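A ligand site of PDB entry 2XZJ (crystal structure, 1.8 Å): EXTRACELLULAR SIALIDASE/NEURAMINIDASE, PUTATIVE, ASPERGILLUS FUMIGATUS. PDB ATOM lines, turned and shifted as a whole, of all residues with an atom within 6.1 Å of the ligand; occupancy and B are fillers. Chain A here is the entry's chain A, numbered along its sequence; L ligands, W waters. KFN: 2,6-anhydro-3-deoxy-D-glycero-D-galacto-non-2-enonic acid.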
ATOM      1  N   ARG A  39       7.126  30.339   4.237  1.00  0.00           N
ATOM      2  CA  ARG A  39       7.171  28.889   4.083  1.00  0.00           C
ATOM      3  C   ARG A  39       7.362  28.519   2.604  1.00  0.00           C
ATOM      4  O   ARG A  39       7.335  29.383   1.702  1.00  0.00           O
ATOM      5  CB  ARG A  39       5.904  28.211   4.625  1.00  0.00           C
ATOM      6  CG  ARG A  39       5.717  28.227   6.135  1.00  0.00           C
ATOM      7  CD  ARG A  39       4.814  27.086   6.568  1.00  0.00           C
ATOM      8  NE  ARG A  39       5.375  25.841   6.079  1.00  0.00           N
ATOM      9  CZ  ARG A  39       4.687  24.748   5.796  1.00  0.00           C
ATOM     10  NH1 ARG A  39       3.367  24.697   5.970  1.00  0.00           N
ATOM     11  NH2 ARG A  39       5.339  23.686   5.328  1.00  0.00           N
ATOM     12  N   ILE A  40       7.581  27.230   2.367  1.00  0.00           N
ATOM     13  CA  ILE A  40       7.566  26.684   1.000  1.00  0.00           C
ATOM     14  C   ILE A  40       8.661  27.329   0.127  1.00  0.00           C
ATOM     15  O   ILE A  40       8.371  28.084  -0.825  1.00  0.00           O
ATOM     16  CB  ILE A  40       6.116  26.762   0.355  1.00  0.00           C
ATOM     17  CG1 ILE A  40       4.989  26.474   1.364  1.00  0.00           C
ATOM     18  CG2 ILE A  40       6.008  25.841  -0.854  1.00  0.00           C
ATOM     19  CD1 ILE A  40       5.109  25.147   2.147  1.00  0.00           C
ATOM     20  N   GLU A  56       6.770  31.375  -0.098  1.00  0.00           N
ATOM     21  CA  GLU A  56       5.444  31.867   0.154  1.00  0.00           C
ATOM     22  C   GLU A  56       5.508  32.876   1.312  1.00  0.00           C
ATOM     23  O   GLU A  56       5.989  32.553   2.401  1.00  0.00           O
ATOM     24  CB  GLU A  56       4.534  30.695   0.510  1.00  0.00           C
ATOM     25  CG  GLU A  56       3.899  30.015  -0.681  1.00  0.00           C
ATOM     26  CD  GLU A  56       3.025  28.848  -0.261  1.00  0.00           C
ATOM     27  OE1 GLU A  56       2.413  28.920   0.834  1.00  0.00           O
ATOM     28  OE2 GLU A  56       2.942  27.868  -1.025  1.00  0.00           O
ATOM     29  N   ARG A  58       3.374  34.406   3.831  1.00  0.00           N
ATOM     30  CA  ARG A  58       2.063  34.134   4.427  1.00  0.00           C
ATOM     31  C   ARG A  58       1.717  35.281   5.337  1.00  0.00           C
ATOM     32  O   ARG A  58       2.353  35.491   6.389  1.00  0.00           O
ATOM     33  CB  ARG A  58       2.070  32.779   5.138  1.00  0.00           C
ATOM     34  CG  ARG A  58       2.504  31.641   4.203  1.00  0.00           C
ATOM     35  CD  ARG A  58       2.248  30.245   4.780  1.00  0.00           C
ATOM     36  NE  ARG A  58       2.263  29.249   3.701  1.00  0.00           N
ATOM     37  CZ  ARG A  58       1.951  27.971   3.856  1.00  0.00           C
ATOM     38  NH1 ARG A  58       1.618  27.509   5.049  1.00  0.00           N
ATOM     39  NH2 ARG A  58       1.989  27.165   2.785  1.00  0.00           N
ATOM     40  N   ASP A  64      -1.846  27.395   5.398  1.00  0.00           N
ATOM     41  CA  ASP A  64      -1.616  27.163   3.965  1.00  0.00           C
ATOM     42  C   ASP A  64      -2.563  27.963   3.077  1.00  0.00           C
ATOM     43  O   ASP A  64      -2.348  28.094   1.874  1.00  0.00           O
ATOM     44  CB  ASP A  64      -1.824  25.679   3.614  1.00  0.00           C
ATOM     45  CG  ASP A  64      -0.954  24.733   4.405  1.00  0.00           C
ATOM     46  OD1 ASP A  64       0.071  25.129   4.987  1.00  0.00           O
ATOM     47  OD2 ASP A  64      -1.328  23.543   4.448  1.00  0.00           O
ATOM     48  N   ASN A 104       3.320  27.501  -3.920  1.00  0.00           N
ATOM     49  CA  ASN A 104       3.952  26.341  -4.502  1.00  0.00           C
ATOM     50  C   ASN A 104       5.013  26.734  -5.538  1.00  0.00           C
ATOM     51  O   ASN A 104       4.964  26.235  -6.648  1.00  0.00           O
ATOM     52  CB  ASN A 104       2.902  25.441  -5.153  1.00  0.00           C
ATOM     53  CG  ASN A 104       2.170  24.578  -4.165  1.00  0.00           C
ATOM     54  OD1 ASN A 104       1.283  25.044  -3.457  1.00  0.00           O
ATOM     55  ND2 ASN A 104       2.555  23.298  -4.094  1.00  0.00           N
ATOM     56  N   GLN A 128      -8.070  23.747   1.462  1.00  0.00           N
ATOM     57  CA  GLN A 128      -8.013  22.318   1.181  1.00  0.00           C
ATOM     58  C   GLN A 128      -9.065  21.505   1.954  1.00  0.00           C
ATOM     59  O   GLN A 128      -9.769  20.652   1.380  1.00  0.00           O
ATOM     60  CB  GLN A 128      -6.606  21.792   1.491  1.00  0.00           C
ATOM     61  CG  GLN A 128      -6.365  20.345   1.022  1.00  0.00           C
ATOM     62  CD  GLN A 128      -4.936  19.881   1.152  1.00  0.00           C
ATOM     63  OE1 GLN A 128      -4.100  20.521   1.814  1.00  0.00           O
ATOM     64  NE2 GLN A 128      -4.627  18.739   0.516  1.00  0.00           N
ATOM     65  N   ARG A 151      -7.961  24.423  -7.317  1.00  0.00           N
ATOM     66  CA  ARG A 151      -6.600  24.877  -7.422  1.00  0.00           C
ATOM     67  C   ARG A 151      -6.190  25.035  -8.881  1.00  0.00           C
ATOM     68  O   ARG A 151      -6.353  24.108  -9.702  1.00  0.00           O
ATOM     69  CB  ARG A 151      -5.665  23.957  -6.654  1.00  0.00           C
ATOM     70  CG  ARG A 151      -5.902  24.027  -5.168  1.00  0.00           C
ATOM     71  CD  ARG A 151      -4.948  25.036  -4.522  1.00  0.00           C
ATOM     72  NE  ARG A 151      -3.623  24.426  -4.409  1.00  0.00           N
ATOM     73  CZ  ARG A 151      -2.567  24.973  -3.830  1.00  0.00           C
ATOM     74  NH1 ARG A 151      -2.638  26.176  -3.286  1.00  0.00           N
ATOM     75  NH2 ARG A 151      -1.416  24.300  -3.797  1.00  0.00           N
ATOM     76  N   TRP A 182      -8.329  19.878  -5.681  1.00  0.00           N
ATOM     77  CA  TRP A 182      -6.979  20.098  -5.145  1.00  0.00           C
ATOM     78  C   TRP A 182      -5.947  19.841  -6.251  1.00  0.00           C
ATOM     79  O   TRP A 182      -6.177  19.003  -7.126  1.00  0.00           O
ATOM     80  CB  TRP A 182      -6.662  19.230  -3.921  1.00  0.00           C
ATOM     81  CG  TRP A 182      -5.330  19.622  -3.297  1.00  0.00           C
ATOM     82  CD1 TRP A 182      -4.162  18.914  -3.325  1.00  0.00           C
ATOM     83  CD2 TRP A 182      -5.041  20.843  -2.602  1.00  0.00           C
ATOM     84  NE1 TRP A 182      -3.166  19.612  -2.690  1.00  0.00           N
ATOM     85  CE2 TRP A 182      -3.685  20.799  -2.230  1.00  0.00           C
ATOM     86  CE3 TRP A 182      -5.809  21.970  -2.251  1.00  0.00           C
ATOM     87  CZ2 TRP A 182      -3.068  21.840  -1.524  1.00  0.00           C
ATOM     88  CZ3 TRP A 182      -5.187  23.002  -1.555  1.00  0.00           C
ATOM     89  CH2 TRP A 182      -3.843  22.927  -1.200  1.00  0.00           C
ATOM     90  N   ALA A 184      -1.331  20.632  -6.870  1.00  0.00           N
ATOM     91  CA  ALA A 184      -0.080  21.183  -6.412  1.00  0.00           C
ATOM     92  C   ALA A 184       0.910  21.068  -7.567  1.00  0.00           C
ATOM     93  O   ALA A 184       0.893  20.071  -8.293  1.00  0.00           O
ATOM     94  CB  ALA A 184       0.424  20.426  -5.188  1.00  0.00           C
ATOM     95  N   ALA A 228       1.137  14.068  -4.272  1.00  0.00           N
ATOM     96  CA  ALA A 228       0.748  15.476  -4.504  1.00  0.00           C
ATOM     97  C   ALA A 228       1.986  16.376  -4.631  1.00  0.00           C
ATOM     98  O   ALA A 228       2.033  17.267  -5.480  1.00  0.00           O
ATOM     99  CB  ALA A 228      -0.149  15.961  -3.367  1.00  0.00           C
ATOM    100  N   GLU A 229       2.992  16.147  -3.768  1.00  0.00           N
ATOM    101  CA  GLU A 229       4.228  16.954  -3.790  1.00  0.00           C
ATOM    102  C   GLU A 229       5.421  16.129  -4.261  1.00  0.00           C
ATOM    103  O   GLU A 229       5.969  15.338  -3.496  1.00  0.00           O
ATOM    104  CB  GLU A 229       4.493  17.578  -2.413  1.00  0.00           C
ATOM    105  CG  GLU A 229       3.464  18.619  -2.009  1.00  0.00           C
ATOM    106  CD  GLU A 229       3.803  19.268  -0.670  1.00  0.00           C
ATOM    107  OE1 GLU A 229       4.573  18.672   0.117  1.00  0.00           O
ATOM    108  OE2 GLU A 229       3.319  20.386  -0.436  1.00  0.00           O
ATOM    109  N   ARG A 245       6.596  12.926  -1.821  1.00  0.00           N
ATOM    110  CA  ARG A 245       6.116  12.873  -0.433  1.00  0.00           C
ATOM    111  C   ARG A 245       5.082  11.753  -0.289  1.00  0.00           C
ATOM    112  O   ARG A 245       4.193  11.637  -1.143  1.00  0.00           O
ATOM    113  CB  ARG A 245       5.480  14.230  -0.095  1.00  0.00           C
ATOM    114  CG  ARG A 245       4.749  14.303   1.227  1.00  0.00           C
ATOM    115  CD  ARG A 245       4.228  15.711   1.421  1.00  0.00           C
ATOM    116  NE  ARG A 245       3.177  15.761   2.431  1.00  0.00           N
ATOM    117  CZ  ARG A 245       2.791  16.884   3.047  1.00  0.00           C
ATOM    118  NH1 ARG A 245       3.395  18.044   2.756  1.00  0.00           N
ATOM    119  NH2 ARG A 245       1.813  16.832   3.943  1.00  0.00           N
ATOM    120  N   ALA A 275       5.939  12.491   6.097  1.00  0.00           N
ATOM    121  CA  ALA A 275       4.905  13.119   5.252  1.00  0.00           C
ATOM    122  C   ALA A 275       5.194  14.620   5.156  1.00  0.00           C
ATOM    123  O   ALA A 275       4.479  15.473   5.695  1.00  0.00           O
ATOM    124  CB  ALA A 275       3.483  12.860   5.760  1.00  0.00           C
ATOM    125  N   CYS A 276       6.306  14.934   4.495  1.00  0.00           N
ATOM    126  CA  CYS A 276       6.695  16.320   4.268  1.00  0.00           C
ATOM    127  C   CYS A 276       7.352  16.415   2.887  1.00  0.00           C
ATOM    128  O   CYS A 276       7.743  15.398   2.320  1.00  0.00           O
ATOM    129  CB  CYS A 276       7.666  16.741   5.373  1.00  0.00           C
ATOM    130  SG  CYS A 276       8.283  18.475   5.357  1.00  0.00           S
ATOM    131  N   ARG A 302       9.601  16.615  11.562  1.00  0.00           N
ATOM    132  CA  ARG A 302      10.203  17.429  10.495  1.00  0.00           C
ATOM    133  C   ARG A 302      11.524  18.050  10.922  1.00  0.00           C
ATOM    134  O   ARG A 302      12.098  18.805  10.161  1.00  0.00           O
ATOM    135  CB  ARG A 302       9.241  18.495   9.977  1.00  0.00           C
ATOM    136  CG  ARG A 302       8.131  17.900   9.118  1.00  0.00           C
ATOM    137  CD  ARG A 302       7.099  18.943   8.773  1.00  0.00           C
ATOM    138  NE  ARG A 302       5.999  18.340   8.038  1.00  0.00           N
ATOM    139  CZ  ARG A 302       5.136  19.022   7.299  1.00  0.00           C
ATOM    140  NH1 ARG A 302       5.232  20.352   7.184  1.00  0.00           N
ATOM    141  NH2 ARG A 302       4.166  18.377   6.668  1.00  0.00           N
ATOM    142  N   TYR A 338      10.127  21.783   4.813  1.00  0.00           N
ATOM    143  CA  TYR A 338      10.392  21.888   3.362  1.00  0.00           C
ATOM    144  C   TYR A 338      11.775  22.441   3.074  1.00  0.00           C
ATOM    145  O   TYR A 338      12.322  23.223   3.872  1.00  0.00           O
ATOM    146  CB  TYR A 338       9.357  22.821   2.707  1.00  0.00           C
ATOM    147  CG  TYR A 338       7.966  22.228   2.535  1.00  0.00           C
ATOM    148  CD1 TYR A 338       7.361  21.491   3.551  1.00  0.00           C
ATOM    149  CD2 TYR A 338       7.258  22.417   1.346  1.00  0.00           C
ATOM    150  CE1 TYR A 338       6.084  20.940   3.388  1.00  0.00           C
ATOM    151  CE2 TYR A 338       5.982  21.886   1.175  1.00  0.00           C
ATOM    152  CZ  TYR A 338       5.405  21.152   2.202  1.00  0.00           C
ATOM    153  OH  TYR A 338       4.150  20.634   2.029  1.00  0.00           O
ATOM    154  N   GLU A 354      12.985  25.370   5.831  1.00  0.00           N
ATOM    155  CA  GLU A 354      12.044  25.987   6.752  1.00  0.00           C
ATOM    156  C   GLU A 354      12.511  25.896   8.223  1.00  0.00           C
ATOM    157  O   GLU A 354      13.233  24.980   8.617  1.00  0.00           O
ATOM    158  CB  GLU A 354      10.644  25.391   6.631  1.00  0.00           C
ATOM    159  CG  GLU A 354      10.036  25.473   5.262  1.00  0.00           C
ATOM    160  CD  GLU A 354       8.662  24.900   5.224  1.00  0.00           C
ATOM    161  OE1 GLU A 354       8.435  23.822   5.851  1.00  0.00           O
ATOM    162  OE2 GLU A 354       7.792  25.491   4.546  1.00  0.00           O
HETATM  163  C1  KFN L   1       2.515  20.954   4.867  1.00  0.00           C
HETATM  164  C3  KFN L   1       2.142  22.735   3.131  1.00  0.00           C
HETATM  165  C4  KFN L   1       1.529  23.245   1.805  1.00  0.00           C
HETATM  166  C5  KFN L   1       0.297  22.374   1.406  1.00  0.00           C
HETATM  167  C6  KFN L   1       0.632  20.864   1.573  1.00  0.00           C
HETATM  168  C7  KFN L   1      -0.557  19.913   1.280  1.00  0.00           C
HETATM  169  C8  KFN L   1      -0.147  18.428   1.215  1.00  0.00           C
HETATM  170  C9  KFN L   1      -1.374  17.532   1.210  1.00  0.00           C
HETATM  171  O5  KFN L   1      -0.129  22.630   0.049  1.00  0.00           O
HETATM  172  O1B KFN L   1       3.287  21.744   5.450  1.00  0.00           O
HETATM  173  O1A KFN L   1       2.256  19.770   5.227  1.00  0.00           O
HETATM  174  O4  KFN L   1       1.226  24.643   1.942  1.00  0.00           O
HETATM  175  O6  KFN L   1       1.047  20.573   2.948  1.00  0.00           O
HETATM  176  C2  KFN L   1       1.881  21.442   3.591  1.00  0.00           C
HETATM  177  O7  KFN L   1      -1.513  20.024   2.332  1.00  0.00           O
HETATM  178  O8  KFN L   1       0.647  18.169   0.065  1.00  0.00           O
HETATM  179  O9  KFN L   1      -2.115  17.715  -0.021  1.00  0.00           O
HETATM  180  O   HOH W   1      -1.133  25.009  -0.104  1.00  0.00           O
HETATM  181  O   HOH W   2       1.937  21.822   7.987  1.00  0.00           O
HETATM  182  O   HOH W   3       2.072  25.359  -0.604  1.00  0.00           O
HETATM  183  O   HOH W   4      -2.930  15.523  -0.960  1.00  0.00           O
HETATM  184  O   HOH W   5      -0.690  19.465   4.985  1.00  0.00           O
HETATM  185  O   HOH W   6       1.053  14.946   0.168  1.00  0.00           O
HETATM  186  O   HOH W   7       1.390  21.427  -1.950  1.00  0.00           O
HETATM  187  O   HOH W   8      -0.200  19.052  -2.305  1.00  0.00           O
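Residues that only touch the ligand: Glu 229 and Ile 40. Hydrophobic or aromatic side chains that line the ligand: Ile 40, Trp 182 and Tyr 338.
N of Tyr 338 lies within hydrogen-bond range of OE1 of Glu 354 (2.8 Å). O of Arg 39 lies within hydrogen-bond range of N of Glu 56, at 2.7 Å. NH1 of Arg 58 lies within salt-bridge range of OD1 of Asp 64. The guanidinium group (NH1) of Arg 245 lies within salt-bridge range of the side-chain carboxylate (OE1) of Glu 229 (3.0 Å). OH of Tyr 338 lies within hydrogen-bond range of OE2 of Glu 229. The guanidinium group of Arg 39 lies within salt-bridge range of the side-chain carboxylate of Asp 64 (3.5 Å). SG of Cys 276 is in hydrogen-bond range of NE of Arg 302, at 3.5 Å. The guanidinium group (NE) of Arg 39 is in salt-bridge range of the side-chain carboxylate (OE2) of Glu 354, 2.9 Å away.
NH1 of Arg 245 is in salt-bridge range of O1A of the ligand, 3.2 Å away. An oxygen (O4) of the ligand sits close to the side-chain carboxylate (OD1) of Asp 64 (3.3 Å). The guanidinium group of Arg 39 is in salt-bridge range of an oxygen (O1B) of the ligand. NE1 of Trp 182 sits at hydrogen-bond distance from O9 of the ligand (3.4 Å). An oxygen (O7) of the ligand is in hydrogen-bond range of the side-chain amide oxygen (OE1) of Gln 128 (2.7 Å). NH2 of Arg 58 is in hydrogen-bond range of O4 of the ligand (2.8 Å). NH2 of Arg 302 lies within salt-bridge range of O1A of the ligand (2.8 Å). The side-chain hydroxyl of Tyr 338 sits close to an oxygen (O6) of the ligand, at 3.2 Å.
Water W8 bridges O8 of the ligand (2.7 Å) and NE1 of Trp 182 (3.0 Å). Water W3 lies within hydrogen-bond range of the side-chain carboxylate of Glu 56 (2.7 Å), an oxygen (O4) of the ligand (2.8 Å) and the side-chain amide oxygen of Asn 104 (3.0 Å). Water W7 lies within hydrogen-bond range of OE2 of Glu 229 (2.7 Å), O5 of the ligand (2.8 Å) and ND2 of Asn 104 (3.1 Å). Water W6 lies within hydrogen-bond range of NE of Arg 245 (3.2 Å) and O8 of the ligand (3.3 Å).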
